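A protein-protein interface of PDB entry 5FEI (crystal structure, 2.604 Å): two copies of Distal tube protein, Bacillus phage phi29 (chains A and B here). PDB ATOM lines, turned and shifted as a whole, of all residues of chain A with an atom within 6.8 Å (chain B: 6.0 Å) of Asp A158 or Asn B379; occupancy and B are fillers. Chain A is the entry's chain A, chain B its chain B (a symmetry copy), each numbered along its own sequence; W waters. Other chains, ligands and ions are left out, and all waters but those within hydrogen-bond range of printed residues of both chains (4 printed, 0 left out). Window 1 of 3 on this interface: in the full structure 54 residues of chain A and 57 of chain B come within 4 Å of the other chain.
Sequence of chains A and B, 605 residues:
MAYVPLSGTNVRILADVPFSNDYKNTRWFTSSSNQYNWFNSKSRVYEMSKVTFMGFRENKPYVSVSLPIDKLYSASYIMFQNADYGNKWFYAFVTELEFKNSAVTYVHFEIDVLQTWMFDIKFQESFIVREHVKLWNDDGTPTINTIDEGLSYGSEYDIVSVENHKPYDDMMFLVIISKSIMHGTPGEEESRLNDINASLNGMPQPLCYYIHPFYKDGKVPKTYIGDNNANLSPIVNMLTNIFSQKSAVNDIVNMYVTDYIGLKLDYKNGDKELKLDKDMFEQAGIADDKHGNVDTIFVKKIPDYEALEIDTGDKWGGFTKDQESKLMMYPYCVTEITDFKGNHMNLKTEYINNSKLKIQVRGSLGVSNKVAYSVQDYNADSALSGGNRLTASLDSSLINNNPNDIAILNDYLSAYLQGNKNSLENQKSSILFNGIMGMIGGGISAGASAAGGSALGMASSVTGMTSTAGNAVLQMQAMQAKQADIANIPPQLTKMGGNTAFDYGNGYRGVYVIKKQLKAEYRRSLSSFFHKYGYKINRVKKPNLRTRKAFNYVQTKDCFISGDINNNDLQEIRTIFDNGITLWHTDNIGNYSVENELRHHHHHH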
ATOM      1  N   GLU A 156      24.120  12.883  -8.871  1.00  0.00           N
ATOM      2  CA  GLU A 156      25.241  13.835  -8.782  1.00  0.00           C
ATOM      3  C   GLU A 156      25.724  14.027  -7.346  1.00  0.00           C
ATOM      4  O   GLU A 156      24.979  13.801  -6.399  1.00  0.00           O
ATOM      5  CB  GLU A 156      24.858  15.204  -9.362  1.00  0.00           C
ATOM      6  CG  GLU A 156      24.450  15.237 -10.854  1.00  0.00           C
ATOM      7  CD  GLU A 156      25.607  14.995 -11.841  1.00  0.00           C
ATOM      8  OE1 GLU A 156      25.347  14.474 -12.949  1.00  0.00           O
ATOM      9  OE2 GLU A 156      26.772  15.326 -11.527  1.00  0.00           O
ATOM     10  N   TYR A 157      26.975  14.456  -7.193  1.00  0.00           N
ATOM     11  CA  TYR A 157      27.511  14.836  -5.893  1.00  0.00           C
ATOM     12  C   TYR A 157      27.534  16.352  -5.714  1.00  0.00           C
ATOM     13  O   TYR A 157      27.598  17.104  -6.686  1.00  0.00           O
ATOM     14  CB  TYR A 157      28.931  14.316  -5.697  1.00  0.00           C
ATOM     15  CG  TYR A 157      29.085  12.814  -5.647  1.00  0.00           C
ATOM     16  CD1 TYR A 157      28.670  12.080  -4.537  1.00  0.00           C
ATOM     17  CD2 TYR A 157      29.699  12.134  -6.687  1.00  0.00           C
ATOM     18  CE1 TYR A 157      28.835  10.709  -4.491  1.00  0.00           C
ATOM     19  CE2 TYR A 157      29.875  10.771  -6.645  1.00  0.00           C
ATOM     20  CZ  TYR A 157      29.441  10.056  -5.555  1.00  0.00           C
ATOM     21  OH  TYR A 157      29.622   8.691  -5.544  1.00  0.00           O
ATOM     22  N   ASP A 158      27.487  16.783  -4.457  1.00  0.00           N
ATOM     23  CA  ASP A 158      27.854  18.143  -4.070  1.00  0.00           C
ATOM     24  C   ASP A 158      29.358  18.230  -3.936  1.00  0.00           C
ATOM     25  O   ASP A 158      29.981  17.348  -3.333  1.00  0.00           O
ATOM     26  CB  ASP A 158      27.212  18.538  -2.745  1.00  0.00           C
ATOM     27  CG  ASP A 158      25.804  19.035  -2.911  1.00  0.00           C
ATOM     28  OD1 ASP A 158      25.442  19.421  -4.041  1.00  0.00           O
ATOM     29  OD2 ASP A 158      25.070  19.062  -1.905  1.00  0.00           O
ATOM     30  N   ILE A 159      29.957  19.275  -4.494  1.00  0.00           N
ATOM     31  CA  ILE A 159      31.359  19.514  -4.194  1.00  0.00           C
ATOM     32  C   ILE A 159      31.429  20.269  -2.882  1.00  0.00           C
ATOM     33  O   ILE A 159      30.914  21.377  -2.753  1.00  0.00           O
ATOM     34  CB  ILE A 159      32.062  20.283  -5.295  1.00  0.00           C
ATOM     35  CG1 ILE A 159      32.048  19.444  -6.568  1.00  0.00           C
ATOM     36  CG2 ILE A 159      33.494  20.621  -4.876  1.00  0.00           C
ATOM     37  CD1 ILE A 159      32.070  20.281  -7.810  1.00  0.00           C
ATOM     38  N   VAL A 160      32.049  19.665  -1.897  1.00  0.00           N
ATOM     39  CA  VAL A 160      31.894  20.211  -0.572  1.00  0.00           C
ATOM     40  C   VAL A 160      33.237  20.768  -0.047  1.00  0.00           C
ATOM     41  O   VAL A 160      33.268  21.511   0.903  1.00  0.00           O
ATOM     42  CB  VAL A 160      31.268  19.135   0.362  1.00  0.00           C
ATOM     43  CG1 VAL A 160      32.331  18.205   0.891  1.00  0.00           C
ATOM     44  CG2 VAL A 160      30.523  19.775   1.484  1.00  0.00           C
ATOM     45  N   SER A 161      34.340  20.453  -0.712  1.00  0.00           N
ATOM     46  CA  SER A 161      35.648  20.953  -0.299  1.00  0.00           C
ATOM     47  C   SER A 161      36.662  20.957  -1.449  1.00  0.00           C
ATOM     48  O   SER A 161      36.794  19.981  -2.174  1.00  0.00           O
ATOM     49  CB  SER A 161      36.191  20.118   0.859  1.00  0.00           C
ATOM     50  OG  SER A 161      37.507  20.523   1.210  1.00  0.00           O
ATOM     51  N   LYS A 515      36.465  17.119  -2.584  1.00  0.00           N
ATOM     52  CA  LYS A 515      35.675  16.186  -1.778  1.00  0.00           C
ATOM     53  C   LYS A 515      34.206  16.303  -2.101  1.00  0.00           C
ATOM     54  O   LYS A 515      33.661  17.407  -2.192  1.00  0.00           O
ATOM     55  CB  LYS A 515      35.926  16.421  -0.292  1.00  0.00           C
ATOM     56  CG  LYS A 515      37.372  16.087   0.067  1.00  0.00           C
ATOM     57  CD  LYS A 515      37.681  16.132   1.539  1.00  0.00           C
ATOM     58  CE  LYS A 515      39.166  15.848   1.739  1.00  0.00           C
ATOM     59  NZ  LYS A 515      39.551  15.798   3.153  1.00  0.00           N
ATOM     60  N   LYS A 516      33.575  15.154  -2.294  1.00  0.00           N
ATOM     61  CA  LYS A 516      32.195  15.086  -2.769  1.00  0.00           C
ATOM     62  C   LYS A 516      31.295  14.234  -1.874  1.00  0.00           C
ATOM     63  O   LYS A 516      31.717  13.174  -1.376  1.00  0.00           O
ATOM     64  CB  LYS A 516      32.167  14.513  -4.185  1.00  0.00           C
ATOM     65  CG  LYS A 516      32.955  15.292  -5.205  1.00  0.00           C
ATOM     66  CD  LYS A 516      33.013  14.498  -6.515  1.00  0.00           C
ATOM     67  CE  LYS A 516      33.625  15.314  -7.636  1.00  0.00           C
ATOM     68  NZ  LYS A 516      33.849  14.474  -8.833  1.00  0.00           N
ATOM     69  N   GLN A 517      30.055  14.676  -1.683  1.00  0.00           N
ATOM     70  CA  GLN A 517      29.070  13.838  -1.009  1.00  0.00           C
ATOM     71  C   GLN A 517      27.690  13.957  -1.651  1.00  0.00           C
ATOM     72  O   GLN A 517      27.408  14.921  -2.366  1.00  0.00           O
ATOM     73  CB  GLN A 517      29.006  14.162   0.489  1.00  0.00           C
ATOM     74  CG  GLN A 517      28.975  15.604   0.863  1.00  0.00           C
ATOM     75  CD  GLN A 517      29.158  15.833   2.375  1.00  0.00           C
ATOM     76  OE1 GLN A 517      28.871  16.922   2.883  1.00  0.00           O
ATOM     77  NE2 GLN A 517      29.622  14.805   3.093  1.00  0.00           N
ATOM     78  N   LEU A 518      26.838  12.963  -1.392  1.00  0.00           N
ATOM     79  CA  LEU A 518      25.532  12.876  -2.037  1.00  0.00           C
ATOM     80  C   LEU A 518      24.636  14.050  -1.621  1.00  0.00           C
ATOM     81  O   LEU A 518      24.841  14.644  -0.571  1.00  0.00           O
ATOM     82  CB  LEU A 518      24.878  11.538  -1.701  1.00  0.00           C
ATOM     83  CG  LEU A 518      24.248  11.419  -0.308  1.00  0.00           C
ATOM     84  CD1 LEU A 518      23.724  10.011  -0.093  1.00  0.00           C
ATOM     85  CD2 LEU A 518      25.235  11.787   0.772  1.00  0.00           C
ATOM     86  N   LYS A 519      23.653  14.385  -2.452  1.00  0.00           N
ATOM     87  CA  LYS A 519      22.785  15.541  -2.205  1.00  0.00           C
ATOM     88  C   LYS A 519      21.916  15.407  -0.946  1.00  0.00           C
ATOM     89  O   LYS A 519      21.623  14.302  -0.497  1.00  0.00           O
ATOM     90  CB  LYS A 519      21.865  15.759  -3.407  1.00  0.00           C
ATOM     91  CG  LYS A 519      22.565  15.817  -4.751  1.00  0.00           C
ATOM     92  CD  LYS A 519      23.252  17.141  -4.952  1.00  0.00           C
ATOM     93  CE  LYS A 519      23.755  17.290  -6.377  1.00  0.00           C
ATOM     94  NZ  LYS A 519      24.491  18.577  -6.508  1.00  0.00           N
ATOM     95  N   ALA A 520      21.481  16.535  -0.398  1.00  0.00           N
ATOM     96  CA  ALA A 520      20.620  16.537   0.789  1.00  0.00           C
ATOM     97  C   ALA A 520      19.429  15.579   0.658  1.00  0.00           C
ATOM     98  O   ALA A 520      19.094  14.843   1.595  1.00  0.00           O
ATOM     99  CB  ALA A 520      20.129  17.940   1.076  1.00  0.00           C
ATOM    100  N   ARG A 523      20.644  12.073   1.259  1.00  0.00           N
ATOM    101  CA  ARG A 523      21.106  11.969   2.636  1.00  0.00           C
ATOM    102  C   ARG A 523      19.901  11.753   3.561  1.00  0.00           C
ATOM    103  O   ARG A 523      19.893  10.806   4.351  1.00  0.00           O
ATOM    104  CB  ARG A 523      21.893  13.219   3.042  1.00  0.00           C
ATOM    105  CG  ARG A 523      22.227  13.310   4.533  1.00  0.00           C
ATOM    106  CD  ARG A 523      22.711  14.717   4.924  1.00  0.00           C
ATOM    107  NE  ARG A 523      23.773  15.171   4.027  1.00  0.00           N
ATOM    108  CZ  ARG A 523      25.024  14.703   4.036  1.00  0.00           C
ATOM    109  NH1 ARG A 523      25.389  13.752   4.897  1.00  0.00           N
ATOM    110  NH2 ARG A 523      25.914  15.182   3.171  1.00  0.00           N
ATOM    111  N   TYR B 351      20.490  21.512 -10.036  1.00  0.00           N
ATOM    112  CA  TYR B 351      21.720  21.353  -9.263  1.00  0.00           C
ATOM    113  C   TYR B 351      22.664  22.538  -9.476  1.00  0.00           C
ATOM    114  O   TYR B 351      23.792  22.565  -8.979  1.00  0.00           O
ATOM    115  CB  TYR B 351      22.383  20.017  -9.613  1.00  0.00           C
ATOM    116  CG  TYR B 351      21.646  18.812  -9.043  1.00  0.00           C
ATOM    117  CD1 TYR B 351      20.867  18.922  -7.883  1.00  0.00           C
ATOM    118  CD2 TYR B 351      21.713  17.571  -9.669  1.00  0.00           C
ATOM    119  CE1 TYR B 351      20.198  17.808  -7.349  1.00  0.00           C
ATOM    120  CE2 TYR B 351      21.042  16.462  -9.158  1.00  0.00           C
ATOM    121  CZ  TYR B 351      20.290  16.579  -8.000  1.00  0.00           C
ATOM    122  OH  TYR B 351      19.640  15.458  -7.507  1.00  0.00           O
ATOM    123  N   ILE B 352      22.169  23.545 -10.185  1.00  0.00           N
ATOM    124  CA  ILE B 352      22.872  24.808 -10.282  1.00  0.00           C
ATOM    125  C   ILE B 352      22.584  25.618  -9.035  1.00  0.00           C
ATOM    126  O   ILE B 352      21.497  26.157  -8.875  1.00  0.00           O
ATOM    127  CB  ILE B 352      22.435  25.597 -11.526  1.00  0.00           C
ATOM    128  CG1 ILE B 352      22.712  24.779 -12.791  1.00  0.00           C
ATOM    129  CG2 ILE B 352      23.094  26.963 -11.560  1.00  0.00           C
ATOM    130  CD1 ILE B 352      22.025  25.354 -14.019  1.00  0.00           C
ATOM    131  N   ASN B 353      23.564  25.721  -8.153  1.00  0.00           N
ATOM    132  CA  ASN B 353      23.315  26.331  -6.860  1.00  0.00           C
ATOM    133  C   ASN B 353      23.311  27.845  -6.946  1.00  0.00           C
ATOM    134  O   ASN B 353      24.230  28.526  -6.479  1.00  0.00           O
ATOM    135  CB  ASN B 353      24.338  25.845  -5.836  1.00  0.00           C
ATOM    136  CG  ASN B 353      23.950  26.216  -4.434  1.00  0.00           C
ATOM    137  OD1 ASN B 353      22.905  26.814  -4.229  1.00  0.00           O
ATOM    138  ND2 ASN B 353      24.759  25.835  -3.456  1.00  0.00           N
ATOM    139  N   VAL B 375      30.136  26.749 -15.585  1.00  0.00           N
ATOM    140  CA  VAL B 375      29.044  27.131 -14.695  1.00  0.00           C
ATOM    141  C   VAL B 375      29.488  26.757 -13.283  1.00  0.00           C
ATOM    142  O   VAL B 375      29.212  25.672 -12.793  1.00  0.00           O
ATOM    143  CB  VAL B 375      27.705  26.457 -15.088  1.00  0.00           C
ATOM    144  CG1 VAL B 375      26.550  26.982 -14.230  1.00  0.00           C
ATOM    145  CG2 VAL B 375      27.405  26.730 -16.549  1.00  0.00           C
ATOM    146  N   GLN B 376      30.209  27.664 -12.635  1.00  0.00           N
ATOM    147  CA  GLN B 376      30.862  27.336 -11.378  1.00  0.00           C
ATOM    148  C   GLN B 376      29.876  26.955 -10.275  1.00  0.00           C
ATOM    149  O   GLN B 376      30.244  26.296  -9.299  1.00  0.00           O
ATOM    150  CB  GLN B 376      31.723  28.504 -10.907  1.00  0.00           C
ATOM    151  CG  GLN B 376      30.944  29.694 -10.413  1.00  0.00           C
ATOM    152  CD  GLN B 376      31.865  30.848 -10.001  1.00  0.00           C
ATOM    153  OE1 GLN B 376      32.958  31.007 -10.550  1.00  0.00           O
ATOM    154  NE2 GLN B 376      31.422  31.653  -9.035  1.00  0.00           N
ATOM    155  N   ASP B 377      28.620  27.350 -10.426  1.00  0.00           N
ATOM    156  CA  ASP B 377      27.649  27.089  -9.377  1.00  0.00           C
ATOM    157  C   ASP B 377      27.116  25.659  -9.463  1.00  0.00           C
ATOM    158  O   ASP B 377      26.458  25.173  -8.547  1.00  0.00           O
ATOM    159  CB  ASP B 377      26.522  28.104  -9.460  1.00  0.00           C
ATOM    160  CG  ASP B 377      26.981  29.503  -9.089  1.00  0.00           C
ATOM    161  OD1 ASP B 377      27.797  29.634  -8.138  1.00  0.00           O
ATOM    162  OD2 ASP B 377      26.539  30.469  -9.751  1.00  0.00           O
ATOM    163  N   TYR B 378      27.427  24.979 -10.561  1.00  0.00           N
ATOM    164  CA  TYR B 378      26.919  23.634 -10.766  1.00  0.00           C
ATOM    165  C   TYR B 378      27.496  22.649  -9.746  1.00  0.00           C
ATOM    166  O   TYR B 378      28.715  22.504  -9.627  1.00  0.00           O
ATOM    167  CB  TYR B 378      27.216  23.162 -12.182  1.00  0.00           C
ATOM    168  CG  TYR B 378      26.473  21.904 -12.582  1.00  0.00           C
ATOM    169  CD1 TYR B 378      25.073  21.831 -12.471  1.00  0.00           C
ATOM    170  CD2 TYR B 378      27.158  20.802 -13.094  1.00  0.00           C
ATOM    171  CE1 TYR B 378      24.372  20.685 -12.847  1.00  0.00           C
ATOM    172  CE2 TYR B 378      26.470  19.648 -13.487  1.00  0.00           C
ATOM    173  CZ  TYR B 378      25.077  19.594 -13.367  1.00  0.00           C
ATOM    174  OH  TYR B 378      24.397  18.455 -13.764  1.00  0.00           O
ATOM    175  N   ASN B 379      26.599  21.995  -9.004  1.00  0.00           N
ATOM    176  CA  ASN B 379      26.971  21.017  -7.976  1.00  0.00           C
ATOM    177  C   ASN B 379      27.793  21.585  -6.823  1.00  0.00           C
ATOM    178  O   ASN B 379      28.421  20.825  -6.083  1.00  0.00           O
ATOM    179  CB  ASN B 379      27.730  19.832  -8.596  1.00  0.00           C
ATOM    180  CG  ASN B 379      26.803  18.881  -9.362  1.00  0.00           C
ATOM    181  OD1 ASN B 379      25.638  18.715  -9.002  1.00  0.00           O
ATOM    182  ND2 ASN B 379      27.319  18.260 -10.422  1.00  0.00           N
ATOM    183  N   ALA B 380      27.779  22.903  -6.652  1.00  0.00           N
ATOM    184  CA  ALA B 380      28.524  23.529  -5.549  1.00  0.00           C
ATOM    185  C   ALA B 380      27.732  23.455  -4.265  1.00  0.00           C
ATOM    186  O   ALA B 380      26.543  23.744  -4.234  1.00  0.00           O
ATOM    187  CB  ALA B 380      28.859  24.976  -5.858  1.00  0.00           C
ATOM    188  N   ASP B 381      28.392  23.052  -3.194  1.00  0.00           N
ATOM    189  CA  ASP B 381      27.780  23.132  -1.885  1.00  0.00           C
ATOM    190  C   ASP B 381      27.593  24.623  -1.559  1.00  0.00           C
ATOM    191  O   ASP B 381      28.426  25.442  -1.951  1.00  0.00           O
ATOM    192  CB  ASP B 381      28.665  22.447  -0.849  1.00  0.00           C
ATOM    193  CG  ASP B 381      28.078  22.487   0.527  1.00  0.00           C
ATOM    194  OD1 ASP B 381      27.135  21.697   0.794  1.00  0.00           O
ATOM    195  OD2 ASP B 381      28.544  23.316   1.328  1.00  0.00           O
ATOM    196  N   LEU B 384      30.417  26.697  -0.240  1.00  0.00           N
ATOM    197  CA  LEU B 384      31.628  26.738  -1.053  1.00  0.00           C
ATOM    198  C   LEU B 384      31.859  28.120  -1.678  1.00  0.00           C
ATOM    199  O   LEU B 384      30.995  28.659  -2.374  1.00  0.00           O
ATOM    200  CB  LEU B 384      31.562  25.666  -2.136  1.00  0.00           C
ATOM    201  CG  LEU B 384      32.846  25.293  -2.872  1.00  0.00           C
ATOM    202  CD1 LEU B 384      33.801  24.553  -1.947  1.00  0.00           C
ATOM    203  CD2 LEU B 384      32.541  24.456  -4.116  1.00  0.00           C
HETATM  204  O   HOH W   1      31.472  23.638   1.494  1.00  0.00           O
HETATM  205  O   HOH W   2      25.741  16.528 -14.967  1.00  0.00           O
HETATM  206  O   HOH W   3      24.186  21.880  -3.616  1.00  0.00           O
HETATM  207  O   HOH W   4      21.735  13.486  -7.134  1.00  0.00           O
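Asp A158 touches just one residue of chain B: Asn B379.
Of the printed residues of chain B, Lys A519 touches Tyr B351 (3.6 Å) and Asn B379 (2.7 Å).
Of the printed residues of chain A, Tyr B351 touches Glu A156 and Lys A519.
Of chain A, only Glu A156 (3.2 Å), Tyr A157 (3.3 Å), Asp A158 (3.4 Å), Ile A159 (2.7 Å) and Lys A519 (2.7 Å) come within 4 Å of Asn B379.
The nearest residue of chain B that does not touch Asp A158 is Asp B381 (4.3 Å).
The nearest printed residue of chain B that does not touch Lys A519 is Ala B380 (5.4 Å).
Printed residues of chain B that touch a printed residue of chain A: Tyr B351, Asn B379, Asp B381 and Leu B384.
Hydrophobic or aromatic side chains of chain B that line the printed part of chain A: Tyr B351 and Leu B384.
Among the printed residues, pairs that only touch across the chains: Glu A156 with Tyr B351, Asp A158 with Asn B379, Ile A159 with Leu B384, Val A160 with Asp B381 and Lys A519 with Tyr B351.
No position is printed for both chains.
N of Ile A159 lies within hydrogen-bond range of O of Asn B379 (2.7 Å).
N of Asp B381 sits at hydrogen-bond distance from O of Ile A159 (3.1 Å).
The side-chain amide nitrogen (ND2) of Asn B379 lies within hydrogen-bond range of the side-chain carboxylate (OE2) of Glu A156, at 3.2 Å.
NZ of Lys A519 is in hydrogen-bond range of OD1 of Asn B379, 2.7 Å away.
O of Tyr A157 lies close to OD1 of Asn B379.
Water W2 bridges OH of Tyr B378 (2.6 Å) and OE1 of Glu A156 (2.9 Å).
Water W3 bridges OD1 of Asp A158 and O of Ala B380.
Water W1 bridges the backbone carbonyl oxygen of Val A160 (2.8 Å) and the side-chain carboxylate of Asp B381 (3.0 Å).
Water W4 bridges OH of Tyr B351 and N of Glu A156.
The backbone carbonyl oxygen (O) of Tyr B351 sits at hydrogen-bond distance from the backbone NH (N) of Asn B379.
The side-chain amino group (NZ) of Lys A519 is in salt-bridge range of the side-chain carboxylate (OD1) of Asp A158 (2.8 Å).
The backbone carbonyl oxygen (O) of Tyr A157 is in hydrogen-bond range of the side-chain amino group (NZ) of Lys A519, at 3.4 Å.
The backbone NH (N) of Val A160 is in hydrogen-bond range of the backbone carbonyl oxygen (O) of Lys A515 (2.8 Å).
The backbone NH (N) of Asp A158 sits at hydrogen-bond distance from the backbone carbonyl oxygen (O) of Gln A517.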
